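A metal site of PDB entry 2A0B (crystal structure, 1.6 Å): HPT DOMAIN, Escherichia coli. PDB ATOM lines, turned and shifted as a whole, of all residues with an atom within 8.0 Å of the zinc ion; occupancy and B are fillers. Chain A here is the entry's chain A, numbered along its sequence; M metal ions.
The backbone carbonyl oxygen of Leu 11 is in hydrogen-bond range of the backbone NH of His 77 (3.3 Å).
The zinc ion is bound by OE2 of Glu 107, OE2 of Glu 103 and NE2 of His 77.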
ATOM      1  N   LEU A  11       1.863 -38.893  23.040  1.00  0.00           N
ATOM      2  CA  LEU A  11       1.172 -37.662  23.281  1.00  0.00           C
ATOM      3  C   LEU A  11       0.392 -37.730  24.684  1.00  0.00           C
ATOM      4  O   LEU A  11       0.095 -36.643  25.058  1.00  0.00           O
ATOM      5  CB  LEU A  11       0.132 -37.356  22.193  1.00  0.00           C
ATOM      6  CG  LEU A  11       0.764 -37.209  20.736  1.00  0.00           C
ATOM      7  CD1 LEU A  11      -0.362 -36.987  19.772  1.00  0.00           C
ATOM      8  CD2 LEU A  11       1.671 -35.974  20.811  1.00  0.00           C
ATOM      9  N   HIS A  77       2.441 -34.516  26.007  1.00  0.00           N
ATOM     10  CA  HIS A  77       3.385 -33.732  25.129  1.00  0.00           C
ATOM     11  C   HIS A  77       3.122 -32.282  25.166  1.00  0.00           C
ATOM     12  O   HIS A  77       4.054 -31.407  25.131  1.00  0.00           O
ATOM     13  CB  HIS A  77       3.175 -34.312  23.713  1.00  0.00           C
ATOM     14  CG  HIS A  77       3.951 -33.506  22.666  1.00  0.00           C
ATOM     15  ND1 HIS A  77       5.319 -33.447  22.747  1.00  0.00           N
ATOM     16  CD2 HIS A  77       3.496 -32.761  21.669  1.00  0.00           C
ATOM     17  CE1 HIS A  77       5.738 -32.667  21.728  1.00  0.00           C
ATOM     18  NE2 HIS A  77       4.669 -32.247  21.123  1.00  0.00           N
ATOM     19  N   LEU A  78       1.895 -31.772  25.292  1.00  0.00           N
ATOM     20  CA  LEU A  78       1.545 -30.409  25.440  1.00  0.00           C
ATOM     21  C   LEU A  78       2.093 -29.880  26.793  1.00  0.00           C
ATOM     22  O   LEU A  78       2.538 -28.767  26.900  1.00  0.00           O
ATOM     23  CB  LEU A  78       0.073 -30.019  25.330  1.00  0.00           C
ATOM     24  CG  LEU A  78      -0.612 -30.390  23.988  1.00  0.00           C
ATOM     25  CD1 LEU A  78      -2.036 -29.902  23.933  1.00  0.00           C
ATOM     26  CD2 LEU A  78       0.159 -29.651  22.858  1.00  0.00           C
ATOM     27  N   LEU A  81       5.747 -29.300  26.236  1.00  0.00           N
ATOM     28  CA  LEU A  81       5.991 -28.006  25.543  1.00  0.00           C
ATOM     29  C   LEU A  81       5.849 -26.790  26.407  1.00  0.00           C
ATOM     30  O   LEU A  81       6.470 -25.743  26.434  1.00  0.00           O
ATOM     31  CB  LEU A  81       5.024 -27.809  24.341  1.00  0.00           C
ATOM     32  CG  LEU A  81       5.399 -28.569  23.086  1.00  0.00           C
ATOM     33  CD1 LEU A  81       4.300 -28.317  22.073  1.00  0.00           C
ATOM     34  CD2 LEU A  81       6.754 -28.035  22.642  1.00  0.00           C
ATOM     35  N   GLN A  84       8.822 -26.461  28.580  1.00  0.00           N
ATOM     36  CA  GLN A  84       9.944 -25.758  27.892  1.00  0.00           C
ATOM     37  C   GLN A  84       9.689 -24.290  27.761  1.00  0.00           C
ATOM     38  O   GLN A  84      10.591 -23.461  28.054  1.00  0.00           O
ATOM     39  CB  GLN A  84      10.116 -26.384  26.488  1.00  0.00           C
ATOM     40  CG  GLN A  84      10.637 -27.798  26.529  1.00  0.00           C
ATOM     41  CD  GLN A  84      10.426 -28.596  25.256  1.00  0.00           C
ATOM     42  OE1 GLN A  84      10.637 -29.799  25.260  1.00  0.00           O
ATOM     43  NE2 GLN A  84       9.903 -28.048  24.175  1.00  0.00           N
ATOM     44  N   GLU A  99       9.401 -21.225  18.122  1.00  0.00           N
ATOM     45  CA  GLU A  99       9.158 -22.496  17.453  1.00  0.00           C
ATOM     46  C   GLU A  99       8.227 -23.358  18.374  1.00  0.00           C
ATOM     47  O   GLU A  99       7.270 -23.915  17.842  1.00  0.00           O
ATOM     48  CB  GLU A  99      10.381 -23.320  17.113  1.00  0.00           C
ATOM     49  CG  GLU A  99      10.072 -24.521  16.226  1.00  0.00           C
ATOM     50  CD  GLU A  99      10.954 -24.675  15.004  1.00  0.00           C
ATOM     51  OE1 GLU A  99      11.690 -23.724  14.626  1.00  0.00           O
ATOM     52  OE2 GLU A  99      11.037 -25.762  14.371  1.00  0.00           O
ATOM     53  N   TRP A 100       8.548 -23.335  19.679  1.00  0.00           N
ATOM     54  CA  TRP A 100       7.636 -24.176  20.532  1.00  0.00           C
ATOM     55  C   TRP A 100       6.278 -23.569  20.582  1.00  0.00           C
ATOM     56  O   TRP A 100       5.309 -24.408  20.612  1.00  0.00           O
ATOM     57  CB  TRP A 100       8.273 -24.136  21.936  1.00  0.00           C
ATOM     58  CG  TRP A 100       9.562 -24.877  22.059  1.00  0.00           C
ATOM     59  CD1 TRP A 100      10.047 -25.911  21.347  1.00  0.00           C
ATOM     60  CD2 TRP A 100      10.608 -24.542  22.989  1.00  0.00           C
ATOM     61  NE1 TRP A 100      11.284 -26.301  21.787  1.00  0.00           N
ATOM     62  CE2 TRP A 100      11.646 -25.442  22.807  1.00  0.00           C
ATOM     63  CE3 TRP A 100      10.668 -23.567  23.997  1.00  0.00           C
ATOM     64  CZ2 TRP A 100      12.813 -25.445  23.570  1.00  0.00           C
ATOM     65  CZ3 TRP A 100      11.865 -23.546  24.734  1.00  0.00           C
ATOM     66  CH2 TRP A 100      12.881 -24.452  24.527  1.00  0.00           C
ATOM     67  N   GLU A 102       4.733 -21.896  18.054  1.00  0.00           N
ATOM     68  CA  GLU A 102       4.072 -22.323  16.836  1.00  0.00           C
ATOM     69  C   GLU A 102       3.748 -23.796  16.806  1.00  0.00           C
ATOM     70  O   GLU A 102       2.683 -24.171  16.260  1.00  0.00           O
ATOM     71  CB  GLU A 102       5.113 -22.027  15.696  1.00  0.00           C
ATOM     72  CG  GLU A 102       4.491 -22.353  14.340  1.00  0.00           C
ATOM     73  CD  GLU A 102       3.303 -21.561  13.885  1.00  0.00           C
ATOM     74  OE1 GLU A 102       2.989 -20.417  14.304  1.00  0.00           O
ATOM     75  OE2 GLU A 102       2.596 -22.143  13.028  1.00  0.00           O
ATOM     76  N   GLU A 103       4.561 -24.697  17.278  1.00  0.00           N
ATOM     77  CA  GLU A 103       4.352 -26.111  17.385  1.00  0.00           C
ATOM     78  C   GLU A 103       3.047 -26.377  18.206  1.00  0.00           C
ATOM     79  O   GLU A 103       2.182 -27.098  17.752  1.00  0.00           O
ATOM     80  CB  GLU A 103       5.508 -26.783  18.064  1.00  0.00           C
ATOM     81  CG  GLU A 103       5.342 -28.268  18.104  1.00  0.00           C
ATOM     82  CD  GLU A 103       6.447 -28.933  18.847  1.00  0.00           C
ATOM     83  OE1 GLU A 103       7.604 -28.392  19.014  1.00  0.00           O
ATOM     84  OE2 GLU A 103       6.307 -30.097  19.304  1.00  0.00           O
ATOM     85  N   MET A 104       3.032 -25.679  19.339  1.00  0.00           N
ATOM     86  CA  MET A 104       1.775 -25.789  20.154  1.00  0.00           C
ATOM     87  C   MET A 104       0.560 -25.341  19.406  1.00  0.00           C
ATOM     88  O   MET A 104      -0.487 -26.030  19.413  1.00  0.00           O
ATOM     89  CB  MET A 104       1.900 -24.859  21.395  1.00  0.00           C
ATOM     90  CG  MET A 104       0.567 -24.891  22.176  1.00  0.00           C
ATOM     91  SD  MET A 104       0.772 -25.905  23.677  1.00  0.00           S
ATOM     92  CE  MET A 104       1.898 -24.770  24.505  1.00  0.00           C
ATOM     93  N   GLU A 106      -0.064 -25.177  16.216  1.00  0.00           N
ATOM     94  CA  GLU A 106      -0.420 -26.061  15.114  1.00  0.00           C
ATOM     95  C   GLU A 106      -0.970 -27.395  15.558  1.00  0.00           C
ATOM     96  O   GLU A 106      -1.746 -27.987  14.788  1.00  0.00           O
ATOM     97  CB  GLU A 106       0.800 -26.362  14.167  1.00  0.00           C
ATOM     98  CG  GLU A 106       1.186 -25.110  13.377  1.00  0.00           C
ATOM     99  CD  GLU A 106       2.418 -25.340  12.460  1.00  0.00           C
ATOM    100  OE1 GLU A 106       2.736 -26.477  12.127  1.00  0.00           O
ATOM    101  OE2 GLU A 106       2.994 -24.289  12.166  1.00  0.00           O
ATOM    102  N   GLU A 107      -0.584 -27.985  16.714  1.00  0.00           N
ATOM    103  CA  GLU A 107      -0.947 -29.317  17.035  1.00  0.00           C
ATOM    104  C   GLU A 107      -2.031 -29.476  18.218  1.00  0.00           C
ATOM    105  O   GLU A 107      -2.374 -30.661  18.220  1.00  0.00           O
ATOM    106  CB  GLU A 107       0.213 -30.119  17.520  1.00  0.00           C
ATOM    107  CG  GLU A 107       0.674 -29.743  18.950  1.00  0.00           C
ATOM    108  CD  GLU A 107       1.755 -30.669  19.333  1.00  0.00           C
ATOM    109  OE1 GLU A 107       1.680 -31.893  19.479  1.00  0.00           O
ATOM    110  OE2 GLU A 107       2.883 -30.094  19.465  1.00  0.00           O
ATOM    111  N   TRP A 108      -2.313 -28.408  18.869  1.00  0.00           N
ATOM    112  CA  TRP A 108      -3.107 -28.849  20.090  1.00  0.00           C
ATOM    113  C   TRP A 108      -4.476 -29.451  19.761  1.00  0.00           C
ATOM    114  O   TRP A 108      -4.782 -30.388  20.542  1.00  0.00           O
ATOM    115  CB  TRP A 108      -3.221 -27.641  21.004  1.00  0.00           C
ATOM    116  CG  TRP A 108      -4.103 -26.546  20.591  1.00  0.00           C
ATOM    117  CD1 TRP A 108      -3.808 -25.399  19.894  1.00  0.00           C
ATOM    118  CD2 TRP A 108      -5.540 -26.453  20.774  1.00  0.00           C
ATOM    119  NE1 TRP A 108      -4.866 -24.603  19.671  1.00  0.00           N
ATOM    120  CE2 TRP A 108      -5.982 -25.291  20.236  1.00  0.00           C
ATOM    121  CE3 TRP A 108      -6.403 -27.386  21.431  1.00  0.00           C
ATOM    122  CZ2 TRP A 108      -7.320 -24.859  20.236  1.00  0.00           C
ATOM    123  CZ3 TRP A 108      -7.736 -26.963  21.433  1.00  0.00           C
ATOM    124  CH2 TRP A 108      -8.170 -25.767  20.869  1.00  0.00           C
ATOM    125  N   ASP A 111      -3.849 -33.170  19.235  1.00  0.00           N
ATOM    126  CA  ASP A 111      -3.588 -33.876  20.463  1.00  0.00           C
ATOM    127  C   ASP A 111      -4.977 -34.063  21.222  1.00  0.00           C
ATOM    128  O   ASP A 111      -5.045 -35.208  21.679  1.00  0.00           O
ATOM    129  CB  ASP A 111      -2.690 -33.034  21.368  1.00  0.00           C
ATOM    130  CG  ASP A 111      -1.211 -33.022  21.061  1.00  0.00           C
ATOM    131  OD1 ASP A 111      -0.950 -32.848  19.820  1.00  0.00           O
ATOM    132  OD2 ASP A 111      -0.263 -33.235  21.825  1.00  0.00           O
HETATM  133 ZN    ZN M   1       4.567 -31.224  19.309  1.00  0.00          ZN
